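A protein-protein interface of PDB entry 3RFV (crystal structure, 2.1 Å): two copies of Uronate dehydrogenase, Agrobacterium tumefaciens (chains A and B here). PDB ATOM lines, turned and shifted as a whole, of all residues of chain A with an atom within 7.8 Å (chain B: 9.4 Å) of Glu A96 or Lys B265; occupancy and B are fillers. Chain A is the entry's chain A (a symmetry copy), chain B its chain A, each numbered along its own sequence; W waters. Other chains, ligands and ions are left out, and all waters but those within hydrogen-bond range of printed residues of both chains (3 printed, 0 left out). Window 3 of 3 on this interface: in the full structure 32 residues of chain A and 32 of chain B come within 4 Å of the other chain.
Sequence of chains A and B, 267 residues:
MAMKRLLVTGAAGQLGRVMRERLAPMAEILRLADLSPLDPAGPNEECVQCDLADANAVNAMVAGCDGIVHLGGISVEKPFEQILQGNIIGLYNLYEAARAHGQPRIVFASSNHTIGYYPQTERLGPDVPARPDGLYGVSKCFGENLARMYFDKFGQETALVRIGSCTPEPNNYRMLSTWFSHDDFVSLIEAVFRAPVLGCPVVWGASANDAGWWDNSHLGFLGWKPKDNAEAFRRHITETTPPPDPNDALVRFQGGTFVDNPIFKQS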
ATOM      1  N   ALA A  55      11.363   7.874   0.558  1.00  0.00           N
ATOM      2  CA  ALA A  55      11.619   9.276   0.908  1.00  0.00           C
ATOM      3  C   ALA A  55      12.614   9.953  -0.031  1.00  0.00           C
ATOM      4  O   ALA A  55      12.357  11.049  -0.545  1.00  0.00           O
ATOM      5  CB  ALA A  55      12.077   9.388   2.361  1.00  0.00           C
ATOM      6  N   VAL A  58      11.188  10.394  -3.515  1.00  0.00           N
ATOM      7  CA  VAL A  58      10.250  11.514  -3.473  1.00  0.00           C
ATOM      8  C   VAL A  58      10.976  12.876  -3.445  1.00  0.00           C
ATOM      9  O   VAL A  58      10.627  13.791  -4.192  1.00  0.00           O
ATOM     10  CB  VAL A  58       9.276  11.380  -2.277  1.00  0.00           C
ATOM     11  CG1 VAL A  58       8.405  12.625  -2.143  1.00  0.00           C
ATOM     12  CG2 VAL A  58       8.412  10.142  -2.450  1.00  0.00           C
ATOM     13  N   ASN A  59      11.999  13.000  -2.601  1.00  0.00           N
ATOM     14  CA  ASN A  59      12.812  14.218  -2.586  1.00  0.00           C
ATOM     15  C   ASN A  59      13.288  14.580  -3.996  1.00  0.00           C
ATOM     16  O   ASN A  59      13.100  15.710  -4.458  1.00  0.00           O
ATOM     17  CB  ASN A  59      13.993  14.081  -1.611  1.00  0.00           C
ATOM     18  CG  ASN A  59      14.792  15.379  -1.452  1.00  0.00           C
ATOM     19  OD1 ASN A  59      15.473  15.833  -2.382  1.00  0.00           O
ATOM     20  ND2 ASN A  59      14.724  15.970  -0.266  1.00  0.00           N
ATOM     21  N   VAL A  62      10.516  15.776  -6.381  1.00  0.00           N
ATOM     22  CA  VAL A  62      10.007  17.124  -6.144  1.00  0.00           C
ATOM     23  C   VAL A  62      11.026  18.233  -6.447  1.00  0.00           C
ATOM     24  O   VAL A  62      10.660  19.316  -6.920  1.00  0.00           O
ATOM     25  CB  VAL A  62       9.482  17.241  -4.693  1.00  0.00           C
ATOM     26  CG1 VAL A  62       9.192  18.693  -4.324  1.00  0.00           C
ATOM     27  CG2 VAL A  62       8.234  16.357  -4.512  1.00  0.00           C
ATOM     28  N   GLY A  90       3.436   8.070   2.256  1.00  0.00           N
ATOM     29  CA  GLY A  90       3.654   8.819   1.032  1.00  0.00           C
ATOM     30  C   GLY A  90       3.385  10.314   1.166  1.00  0.00           C
ATOM     31  O   GLY A  90       4.057  11.133   0.538  1.00  0.00           O
ATOM     32  N   LEU A  91       2.391  10.674   1.971  1.00  0.00           N
ATOM     33  CA  LEU A  91       2.061  12.082   2.190  1.00  0.00           C
ATOM     34  C   LEU A  91       3.146  12.769   3.007  1.00  0.00           C
ATOM     35  O   LEU A  91       3.532  13.892   2.716  1.00  0.00           O
ATOM     36  CB  LEU A  91       0.705  12.233   2.900  1.00  0.00           C
ATOM     37  CG  LEU A  91      -0.452  12.670   2.004  1.00  0.00           C
ATOM     38  CD1 LEU A  91      -0.337  14.140   1.641  1.00  0.00           C
ATOM     39  CD2 LEU A  91      -0.482  11.802   0.744  1.00  0.00           C
ATOM     40  N   TYR A  92       3.620  12.094   4.042  1.00  0.00           N
ATOM     41  CA  TYR A  92       4.710  12.627   4.844  1.00  0.00           C
ATOM     42  C   TYR A  92       5.934  12.907   3.970  1.00  0.00           C
ATOM     43  O   TYR A  92       6.537  13.974   4.064  1.00  0.00           O
ATOM     44  CB  TYR A  92       5.061  11.680   5.989  1.00  0.00           C
ATOM     45  CG  TYR A  92       6.344  12.058   6.687  1.00  0.00           C
ATOM     46  CD1 TYR A  92       6.395  13.163   7.540  1.00  0.00           C
ATOM     47  CD2 TYR A  92       7.512  11.318   6.488  1.00  0.00           C
ATOM     48  CE1 TYR A  92       7.574  13.525   8.178  1.00  0.00           C
ATOM     49  CE2 TYR A  92       8.703  11.669   7.126  1.00  0.00           C
ATOM     50  CZ  TYR A  92       8.726  12.780   7.971  1.00  0.00           C
ATOM     51  OH  TYR A  92       9.894  13.142   8.610  1.00  0.00           O
ATOM     52  N   ASN A  93       6.278  11.961   3.103  1.00  0.00           N
ATOM     53  CA  ASN A  93       7.433  12.124   2.218  1.00  0.00           C
ATOM     54  C   ASN A  93       7.252  13.271   1.247  1.00  0.00           C
ATOM     55  O   ASN A  93       8.195  14.014   0.977  1.00  0.00           O
ATOM     56  CB  ASN A  93       7.745  10.823   1.450  1.00  0.00           C
ATOM     57  CG  ASN A  93       8.285   9.733   2.357  1.00  0.00           C
ATOM     58  OD1 ASN A  93       8.745  10.017   3.467  1.00  0.00           O
ATOM     59  ND2 ASN A  93       8.214   8.475   1.905  1.00  0.00           N
ATOM     60  N   LEU A  94       6.048  13.413   0.704  1.00  0.00           N
ATOM     61  CA  LEU A  94       5.778  14.531  -0.192  1.00  0.00           C
ATOM     62  C   LEU A  94       5.964  15.888   0.499  1.00  0.00           C
ATOM     63  O   LEU A  94       6.573  16.796  -0.068  1.00  0.00           O
ATOM     64  CB  LEU A  94       4.368  14.449  -0.781  1.00  0.00           C
ATOM     65  CG  LEU A  94       4.077  15.469  -1.883  1.00  0.00           C
ATOM     66  CD1 LEU A  94       4.768  15.060  -3.190  1.00  0.00           C
ATOM     67  CD2 LEU A  94       2.565  15.632  -2.095  1.00  0.00           C
ATOM     68  N   TYR A  95       5.419  16.027   1.705  1.00  0.00           N
ATOM     69  CA  TYR A  95       5.498  17.297   2.434  1.00  0.00           C
ATOM     70  C   TYR A  95       6.918  17.625   2.928  1.00  0.00           C
ATOM     71  O   TYR A  95       7.350  18.778   2.872  1.00  0.00           O
ATOM     72  CB  TYR A  95       4.422  17.381   3.540  1.00  0.00           C
ATOM     73  CG  TYR A  95       3.125  17.857   2.934  1.00  0.00           C
ATOM     74  CD1 TYR A  95       2.774  19.201   2.966  1.00  0.00           C
ATOM     75  CD2 TYR A  95       2.299  16.975   2.229  1.00  0.00           C
ATOM     76  CE1 TYR A  95       1.603  19.657   2.347  1.00  0.00           C
ATOM     77  CE2 TYR A  95       1.134  17.417   1.610  1.00  0.00           C
ATOM     78  CZ  TYR A  95       0.790  18.757   1.676  1.00  0.00           C
ATOM     79  OH  TYR A  95      -0.360  19.196   1.069  1.00  0.00           O
ATOM     80  N   GLU A  96       7.649  16.610   3.377  1.00  0.00           N
ATOM     81  CA  GLU A  96       9.064  16.787   3.679  1.00  0.00           C
ATOM     82  C   GLU A  96       9.832  17.213   2.427  1.00  0.00           C
ATOM     83  O   GLU A  96      10.646  18.140   2.473  1.00  0.00           O
ATOM     84  CB  GLU A  96       9.656  15.518   4.297  1.00  0.00           C
ATOM     85  CG  GLU A  96       9.413  15.430   5.785  1.00  0.00           C
ATOM     86  CD  GLU A  96       9.927  16.668   6.511  1.00  0.00           C
ATOM     87  OE1 GLU A  96      11.161  16.811   6.628  1.00  0.00           O
ATOM     88  OE2 GLU A  96       9.108  17.512   6.943  1.00  0.00           O
ATOM     89  N   ALA A  97       9.543  16.569   1.297  1.00  0.00           N
ATOM     90  CA  ALA A  97      10.247  16.883   0.059  1.00  0.00           C
ATOM     91  C   ALA A  97      10.009  18.326  -0.379  1.00  0.00           C
ATOM     92  O   ALA A  97      10.947  19.030  -0.784  1.00  0.00           O
ATOM     93  CB  ALA A  97       9.857  15.918  -1.045  1.00  0.00           C
ATOM     94  N   ALA A  98       8.755  18.759  -0.307  1.00  0.00           N
ATOM     95  CA  ALA A  98       8.402  20.133  -0.637  1.00  0.00           C
ATOM     96  C   ALA A  98       9.091  21.104   0.322  1.00  0.00           C
ATOM     97  O   ALA A  98       9.578  22.152  -0.091  1.00  0.00           O
ATOM     98  CB  ALA A  98       6.877  20.330  -0.583  1.00  0.00           C
ATOM     99  N   ARG A  99       9.113  20.755   1.603  1.00  0.00           N
ATOM    100  CA  ARG A  99       9.683  21.635   2.620  1.00  0.00           C
ATOM    101  C   ARG A  99      11.181  21.844   2.357  1.00  0.00           C
ATOM    102  O   ARG A  99      11.721  22.916   2.629  1.00  0.00           O
ATOM    103  CB  ARG A  99       9.454  21.072   4.026  1.00  0.00           C
ATOM    104  CG  ARG A  99       9.900  22.011   5.155  1.00  0.00           C
ATOM    105  CD  ARG A  99       9.458  21.525   6.526  1.00  0.00           C
ATOM    106  NE  ARG A  99      10.169  20.326   6.968  1.00  0.00           N
ATOM    107  CZ  ARG A  99      11.324  20.340   7.632  1.00  0.00           C
ATOM    108  NH1 ARG A  99      11.911  21.499   7.934  1.00  0.00           N
ATOM    109  NH2 ARG A  99      11.894  19.197   7.994  1.00  0.00           N
ATOM    110  N   ALA A 100      11.835  20.818   1.813  1.00  0.00           N
ATOM    111  CA  ALA A 100      13.266  20.878   1.522  1.00  0.00           C
ATOM    112  C   ALA A 100      13.564  21.580   0.199  1.00  0.00           C
ATOM    113  O   ALA A 100      14.705  21.952  -0.065  1.00  0.00           O
ATOM    114  CB  ALA A 100      13.875  19.472   1.534  1.00  0.00           C
ATOM    115  N   HIS A 101      12.543  21.783  -0.627  1.00  0.00           N
ATOM    116  CA  HIS A 101      12.769  22.354  -1.953  1.00  0.00           C
ATOM    117  C   HIS A 101      11.902  23.573  -2.301  1.00  0.00           C
ATOM    118  O   HIS A 101      11.372  23.684  -3.412  1.00  0.00           O
ATOM    119  CB  HIS A 101      12.675  21.267  -3.034  1.00  0.00           C
ATOM    120  CG  HIS A 101      13.707  20.192  -2.886  1.00  0.00           C
ATOM    121  ND1 HIS A 101      14.980  20.308  -3.400  1.00  0.00           N
ATOM    122  CD2 HIS A 101      13.668  18.998  -2.248  1.00  0.00           C
ATOM    123  CE1 HIS A 101      15.676  19.226  -3.098  1.00  0.00           C
ATOM    124  NE2 HIS A 101      14.904  18.416  -2.399  1.00  0.00           N
ATOM    125  N   GLY A 102      11.781  24.499  -1.358  1.00  0.00           N
ATOM    126  CA  GLY A 102      11.144  25.772  -1.648  1.00  0.00           C
ATOM    127  C   GLY A 102       9.637  25.795  -1.446  1.00  0.00           C
ATOM    128  O   GLY A 102       8.984  26.785  -1.770  1.00  0.00           O
ATOM    129  N   GLN A 103       9.089  24.709  -0.912  1.00  0.00           N
ATOM    130  CA  GLN A 103       7.654  24.631  -0.614  1.00  0.00           C
ATOM    131  C   GLN A 103       6.778  24.980  -1.810  1.00  0.00           C
ATOM    132  O   GLN A 103       5.921  25.859  -1.728  1.00  0.00           O
ATOM    133  CB  GLN A 103       7.302  25.525   0.586  1.00  0.00           C
ATOM    134  CG  GLN A 103       7.811  24.960   1.890  1.00  0.00           C
ATOM    135  CD  GLN A 103       7.604  25.875   3.092  1.00  0.00           C
ATOM    136  OE1 GLN A 103       8.113  25.595   4.173  1.00  0.00           O
ATOM    137  NE2 GLN A 103       6.858  26.964   2.911  1.00  0.00           N
ATOM    138  N   ILE A 106       0.913  23.181  -3.467  1.00  0.00           N
ATOM    139  CA  ILE A 106       0.355  21.850  -3.719  1.00  0.00           C
ATOM    140  C   ILE A 106      -1.164  21.850  -3.946  1.00  0.00           C
ATOM    141  O   ILE A 106      -1.923  22.465  -3.188  1.00  0.00           O
ATOM    142  CB  ILE A 106       0.680  20.889  -2.550  1.00  0.00           C
ATOM    143  CG1 ILE A 106       2.193  20.682  -2.429  1.00  0.00           C
ATOM    144  CG2 ILE A 106      -0.046  19.533  -2.718  1.00  0.00           C
ATOM    145  CD1 ILE A 106       2.605  20.052  -1.123  1.00  0.00           C
ATOM    146  N   LEU A 146      -2.257  16.703   7.910  1.00  0.00           N
ATOM    147  CA  LEU A 146      -0.821  16.878   7.721  1.00  0.00           C
ATOM    148  C   LEU A 146      -0.531  18.180   6.972  1.00  0.00           C
ATOM    149  O   LEU A 146       0.288  18.984   7.417  1.00  0.00           O
ATOM    150  CB  LEU A 146      -0.220  15.695   6.962  1.00  0.00           C
ATOM    151  CG  LEU A 146       1.314  15.712   6.863  1.00  0.00           C
ATOM    152  CD1 LEU A 146       1.897  15.233   8.171  1.00  0.00           C
ATOM    153  CD2 LEU A 146       1.820  14.863   5.704  1.00  0.00           C
ATOM    154  N   MET A 149      -1.041  21.201   9.246  1.00  0.00           N
ATOM    155  CA  MET A 149       0.082  21.382  10.163  1.00  0.00           C
ATOM    156  C   MET A 149       1.272  22.045   9.457  1.00  0.00           C
ATOM    157  O   MET A 149       1.874  22.980   9.997  1.00  0.00           O
ATOM    158  CB  MET A 149       0.485  20.045  10.811  1.00  0.00           C
ATOM    159  CG  MET A 149       1.589  20.147  11.867  1.00  0.00           C
ATOM    160  SD  MET A 149       3.242  20.034  11.117  1.00  0.00           S
ATOM    161  CE  MET A 149       3.310  18.273  10.722  1.00  0.00           C
ATOM    162  N   TYR A 150       1.598  21.577   8.251  1.00  0.00           N
ATOM    163  CA  TYR A 150       2.669  22.185   7.465  1.00  0.00           C
ATOM    164  C   TYR A 150       2.387  23.636   7.119  1.00  0.00           C
ATOM    165  O   TYR A 150       3.316  24.459   7.076  1.00  0.00           O
ATOM    166  CB  TYR A 150       3.008  21.367   6.203  1.00  0.00           C
ATOM    167  CG  TYR A 150       3.953  20.229   6.510  1.00  0.00           C
ATOM    168  CD1 TYR A 150       5.325  20.354   6.304  1.00  0.00           C
ATOM    169  CD2 TYR A 150       3.476  19.038   7.040  1.00  0.00           C
ATOM    170  CE1 TYR A 150       6.190  19.310   6.602  1.00  0.00           C
ATOM    171  CE2 TYR A 150       4.322  17.995   7.336  1.00  0.00           C
ATOM    172  CZ  TYR A 150       5.683  18.134   7.117  1.00  0.00           C
ATOM    173  OH  TYR A 150       6.512  17.082   7.428  1.00  0.00           O
ATOM    174  N   PHE A 154       4.988  25.983   8.775  1.00  0.00           N
ATOM    175  CA  PHE A 154       6.024  26.391   7.821  1.00  0.00           C
ATOM    176  C   PHE A 154       5.542  27.319   6.710  1.00  0.00           C
ATOM    177  O   PHE A 154       6.353  27.848   5.950  1.00  0.00           O
ATOM    178  CB  PHE A 154       6.684  25.161   7.178  1.00  0.00           C
ATOM    179  CG  PHE A 154       7.344  24.243   8.161  1.00  0.00           C
ATOM    180  CD1 PHE A 154       8.518  24.621   8.800  1.00  0.00           C
ATOM    181  CD2 PHE A 154       6.801  22.997   8.439  1.00  0.00           C
ATOM    182  CE1 PHE A 154       9.136  23.772   9.701  1.00  0.00           C
ATOM    183  CE2 PHE A 154       7.409  22.141   9.344  1.00  0.00           C
ATOM    184  CZ  PHE A 154       8.581  22.528   9.977  1.00  0.00           C
ATOM    185  N   GLN A 156       3.668  26.303   4.218  1.00  0.00           N
ATOM    186  CA  GLN A 156       3.393  25.507   3.018  1.00  0.00           C
ATOM    187  C   GLN A 156       1.921  25.661   2.639  1.00  0.00           C
ATOM    188  O   GLN A 156       1.051  25.425   3.465  1.00  0.00           O
ATOM    189  CB  GLN A 156       3.692  24.030   3.282  1.00  0.00           C
ATOM    190  CG  GLN A 156       3.197  23.103   2.173  1.00  0.00           C
ATOM    191  CD  GLN A 156       3.994  23.243   0.893  1.00  0.00           C
ATOM    192  OE1 GLN A 156       5.202  23.000   0.876  1.00  0.00           O
ATOM    193  NE2 GLN A 156       3.325  23.643  -0.190  1.00  0.00           N
ATOM    194  N   GLU B  77       6.129  15.003  20.673  1.00  0.00           N
ATOM    195  CA  GLU B  77       6.581  15.105  19.293  1.00  0.00           C
ATOM    196  C   GLU B  77       7.833  14.249  19.098  1.00  0.00           C
ATOM    197  O   GLU B  77       8.772  14.326  19.884  1.00  0.00           O
ATOM    198  CB  GLU B  77       6.852  16.557  18.905  1.00  0.00           C
ATOM    199  CG  GLU B  77       7.153  16.754  17.422  1.00  0.00           C
ATOM    200  CD  GLU B  77       5.942  16.498  16.521  1.00  0.00           C
ATOM    201  OE1 GLU B  77       4.843  16.212  17.056  1.00  0.00           O
ATOM    202  OE2 GLU B  77       6.092  16.600  15.280  1.00  0.00           O
ATOM    203  N   LYS B  78       7.830  13.419  18.060  1.00  0.00           N
ATOM    204  CA  LYS B  78       8.948  12.522  17.799  1.00  0.00           C
ATOM    205  C   LYS B  78       9.074  12.331  16.308  1.00  0.00           C
ATOM    206  O   LYS B  78       8.226  12.811  15.554  1.00  0.00           O
ATOM    207  CB  LYS B  78       8.730  11.181  18.498  1.00  0.00           C
ATOM    208  CG  LYS B  78       9.035  11.220  19.980  1.00  0.00           C
ATOM    209  CD  LYS B  78       9.379   9.839  20.499  1.00  0.00           C
ATOM    210  CE  LYS B  78       9.698   9.853  21.987  1.00  0.00           C
ATOM    211  NZ  LYS B  78      10.866  10.730  22.287  1.00  0.00           N
ATOM    212  N   PRO B  79      10.146  11.656  15.863  1.00  0.00           N
ATOM    213  CA  PRO B  79      10.268  11.401  14.427  1.00  0.00           C
ATOM    214  C   PRO B  79       9.080  10.586  13.913  1.00  0.00           C
ATOM    215  O   PRO B  79       8.488   9.825  14.674  1.00  0.00           O
ATOM    216  CB  PRO B  79      11.559  10.578  14.324  1.00  0.00           C
ATOM    217  CG  PRO B  79      12.353  10.966  15.548  1.00  0.00           C
ATOM    218  CD  PRO B  79      11.330  11.202  16.620  1.00  0.00           C
ATOM    219  N   PHE B  80       8.755  10.751  12.637  1.00  0.00           N
ATOM    220  CA  PHE B  80       7.589  10.102  12.029  1.00  0.00           C
ATOM    221  C   PHE B  80       7.552   8.587  12.253  1.00  0.00           C
ATOM    222  O   PHE B  80       6.512   8.035  12.610  1.00  0.00           O
ATOM    223  CB  PHE B  80       7.533  10.423  10.535  1.00  0.00           C
ATOM    224  CG  PHE B  80       6.333   9.838   9.824  1.00  0.00           C
ATOM    225  CD1 PHE B  80       5.057  10.320  10.072  1.00  0.00           C
ATOM    226  CD2 PHE B  80       6.488   8.818   8.900  1.00  0.00           C
ATOM    227  CE1 PHE B  80       3.950   9.783   9.421  1.00  0.00           C
ATOM    228  CE2 PHE B  80       5.385   8.281   8.247  1.00  0.00           C
ATOM    229  CZ  PHE B  80       4.115   8.773   8.512  1.00  0.00           C
ATOM    230  N   GLU B  81       8.692   7.924  12.064  1.00  0.00           N
ATOM    231  CA  GLU B  81       8.765   6.462  12.168  1.00  0.00           C
ATOM    232  C   GLU B  81       8.199   5.902  13.468  1.00  0.00           C
ATOM    233  O   GLU B  81       7.501   4.883  13.461  1.00  0.00           O
ATOM    234  CB  GLU B  81      10.204   5.967  11.981  1.00  0.00           C
ATOM    235  CG  GLU B  81      10.770   6.176  10.582  1.00  0.00           C
ATOM    236  CD  GLU B  81      11.296   7.594  10.343  1.00  0.00           C
ATOM    237  OE1 GLU B  81      11.208   8.448  11.262  1.00  0.00           O
ATOM    238  OE2 GLU B  81      11.801   7.849   9.224  1.00  0.00           O
ATOM    239  N   GLN B  82       8.503   6.557  14.585  1.00  0.00           N
ATOM    240  CA  GLN B  82       8.028   6.090  15.882  1.00  0.00           C
ATOM    241  C   GLN B  82       6.537   6.376  16.046  1.00  0.00           C
ATOM    242  O   GLN B  82       5.797   5.579  16.618  1.00  0.00           O
ATOM    243  CB  GLN B  82       8.799   6.769  17.011  1.00  0.00           C
ATOM    244  CG  GLN B  82      10.308   6.683  16.867  1.00  0.00           C
ATOM    245  CD  GLN B  82      11.026   7.380  17.999  1.00  0.00           C
ATOM    246  OE1 GLN B  82      10.585   7.335  19.152  1.00  0.00           O
ATOM    247  NE2 GLN B  82      12.141   8.029  17.682  1.00  0.00           N
ATOM    248  N   LEU B 135       3.615  16.333  14.103  1.00  0.00           N
ATOM    249  CA  LEU B 135       3.323  14.955  13.711  1.00  0.00           C
ATOM    250  C   LEU B 135       2.515  14.243  14.791  1.00  0.00           C
ATOM    251  O   LEU B 135       1.609  13.470  14.492  1.00  0.00           O
ATOM    252  CB  LEU B 135       4.613  14.184  13.430  1.00  0.00           C
ATOM    253  CG  LEU B 135       5.416  14.691  12.230  1.00  0.00           C
ATOM    254  CD1 LEU B 135       6.628  13.795  11.977  1.00  0.00           C
ATOM    255  CD2 LEU B 135       4.527  14.764  10.990  1.00  0.00           C
ATOM    256  N   PRO B 262      10.242  21.630  15.624  1.00  0.00           N
ATOM    257  CA  PRO B 262      10.482  21.371  14.200  1.00  0.00           C
ATOM    258  C   PRO B 262       9.990  19.963  13.854  1.00  0.00           C
ATOM    259  O   PRO B 262       9.397  19.308  14.703  1.00  0.00           O
ATOM    260  CB  PRO B 262      12.013  21.428  14.086  1.00  0.00           C
ATOM    261  CG  PRO B 262      12.516  21.037  15.456  1.00  0.00           C
ATOM    262  CD  PRO B 262      11.429  21.368  16.460  1.00  0.00           C
ATOM    263  N   ILE B 263      10.228  19.501  12.633  1.00  0.00           N
ATOM    264  CA  ILE B 263      10.011  18.093  12.334  1.00  0.00           C
ATOM    265  C   ILE B 263      11.256  17.348  12.815  1.00  0.00           C
ATOM    266  O   ILE B 263      12.340  17.518  12.256  1.00  0.00           O
ATOM    267  CB  ILE B 263       9.775  17.839  10.821  1.00  0.00           C
ATOM    268  CG1 ILE B 263       8.557  18.623  10.329  1.00  0.00           C
ATOM    269  CG2 ILE B 263       9.549  16.343  10.548  1.00  0.00           C
ATOM    270  CD1 ILE B 263       7.290  18.319  11.125  1.00  0.00           C
ATOM    271  N   PHE B 264      11.115  16.567  13.878  1.00  0.00           N
ATOM    272  CA  PHE B 264      12.240  15.802  14.401  1.00  0.00           C
ATOM    273  C   PHE B 264      12.596  14.632  13.476  1.00  0.00           C
ATOM    274  O   PHE B 264      11.712  13.995  12.901  1.00  0.00           O
ATOM    275  CB  PHE B 264      11.950  15.294  15.814  1.00  0.00           C
ATOM    276  CG  PHE B 264      11.852  16.385  16.846  1.00  0.00           C
ATOM    277  CD1 PHE B 264      12.799  17.396  16.902  1.00  0.00           C
ATOM    278  CD2 PHE B 264      10.824  16.386  17.778  1.00  0.00           C
ATOM    279  CE1 PHE B 264      12.714  18.393  17.858  1.00  0.00           C
ATOM    280  CE2 PHE B 264      10.732  17.383  18.737  1.00  0.00           C
ATOM    281  CZ  PHE B 264      11.680  18.386  18.778  1.00  0.00           C
ATOM    282  N   LYS B 265      13.893  14.371  13.329  1.00  0.00           N
ATOM    283  CA  LYS B 265      14.397  13.280  12.487  1.00  0.00           C
ATOM    284  C   LYS B 265      15.151  12.231  13.318  1.00  0.00           C
ATOM    285  O   LYS B 265      15.684  12.532  14.391  1.00  0.00           O
ATOM    286  CB  LYS B 265      15.322  13.829  11.402  1.00  0.00           C
ATOM    287  CG  LYS B 265      14.682  14.852  10.466  1.00  0.00           C
ATOM    288  CD  LYS B 265      13.555  14.228   9.668  1.00  0.00           C
ATOM    289  CE  LYS B 265      12.811  15.258   8.824  1.00  0.00           C
ATOM    290  NZ  LYS B 265      13.421  15.488   7.486  1.00  0.00           N
ATOM    291  N   GLN B 266      15.196  10.999  12.823  1.00  0.00           N
ATOM    292  CA  GLN B 266      15.872   9.914  13.540  1.00  0.00           C
ATOM    293  C   GLN B 266      17.390   9.964  13.376  1.00  0.00           C
ATOM    294  O   GLN B 266      17.896  10.131  12.265  1.00  0.00           O
ATOM    295  CB  GLN B 266      15.332   8.551  13.093  1.00  0.00           C
ATOM    296  CG  GLN B 266      14.026   8.163  13.767  1.00  0.00           C
ATOM    297  CD  GLN B 266      13.540   6.788  13.355  1.00  0.00           C
ATOM    298  OE1 GLN B 266      13.758   6.350  12.221  1.00  0.00           O
ATOM    299  NE2 GLN B 266      12.870   6.096  14.276  1.00  0.00           N
HETATM  300  O   HOH W   1      14.147  19.063  10.165  1.00  0.00           O
HETATM  301  O   HOH W   2      10.102  12.575  11.144  1.00  0.00           O
HETATM  302  O   HOH W   3      11.815  21.074  10.868  1.00  0.00           O
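NZ of Lys B265 lies within salt-bridge range of OE1 of Glu A96, at 2.8 Å.
The backbone carbonyl oxygen (O) of Tyr A150 sits at hydrogen-bond distance from the backbone NH (N) of Gln A156 (3.4 Å). The side-chain carboxylate (OE2) of Glu A96 is in hydrogen-bond range of the side-chain hydroxyl (OH) of Tyr A150 (2.7 Å). The side-chain carboxylate (OE2) of Glu B77 is in hydrogen-bond range of the backbone NH (N) of Leu B135. The side-chain carboxylate of Glu A96 lies within salt-bridge range of the guanidinium group of Arg A99 (2.8 Å). NE2 of Gln A103 sits at hydrogen-bond distance from O of Phe A154, at 3.2 Å.
Among the printed residues, pairs that only touch across the chains: Tyr A92 with Phe B80 (3.6 Å), Tyr A92 with Leu B135 (3.9 Å), Tyr A92 with Ile B263 (3.8 Å), Tyr A92 with Lys B265 (3.6 Å), Glu A96 with Ile B263 (3.6 Å), Arg A99 with Ile B263 (3.8 Å), Leu A146 with Leu B135 (3.9 Å), Met A149 with Leu B135 (3.7 Å), Tyr A150 with Ile B263 (3.9 Å) and Phe A154 with Ile B263 (3.8 Å).
Of chain B, only Ile B263 and Lys B265 come within 4 Å of Glu A96. No residue of chain B comes within 4 Å of Ala A97. Ala A98 touches none of the printed residues of chain B. Printed residues of chain A within 4 Å of Ile B263: Tyr A92, Glu A96, Arg A99, Tyr A150 and Phe A154. Printed residues of chain B within 4 Å of Met A149: Leu B135. Printed residues of chain B within 4 Å of Phe A154: Ile B263. Printed residues of chain A within 4 Å of Leu B135: Tyr A92, Leu A146 and Met A149. Of the printed residues of chain B, Leu A146 touches Leu B135 (3.9 Å). Lys B78 touches none of the printed residues of chain A. The nearest residue of chain B that does not touch Glu A96 is Leu B135 (6.7 Å). The nearest residue of chain A that does not touch Lys B265 is Arg A99 (4.04 Å). The nearest printed residue of chain A that does not touch Leu B135 is Tyr A150 (4.7 Å).
Of the 24 printed residues of chain A, 7 touch a printed residue of chain B. Printed residues of chain A that touch a printed residue of chain B: Tyr A92, Glu A96, Arg A99, Leu A146, Met A149, Tyr A150 and Phe A154. Of the 12 printed residues of chain B, 4 touch a printed residue of chain A. Among the printed residues, Asp or Glu carboxylates within 4 Å of a Lys or Arg side-chain nitrogen of the other chain: Glu A96 with Lys B265.
No position is printed for both chains.
Water W2 lies within hydrogen-bond range of OH of Tyr A92, N of Phe B80 and O of Phe B264. Water W3 bridges the backbone NH of Ile B263 (2.8 Å) and the guanidinium group of Arg A99 (3.0 Å). Water W1 bridges the guanidinium group (NH2) of Arg A99 (3.1 Å) and the backbone carbonyl oxygen (O) of Ile B263 (3.2 Å).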
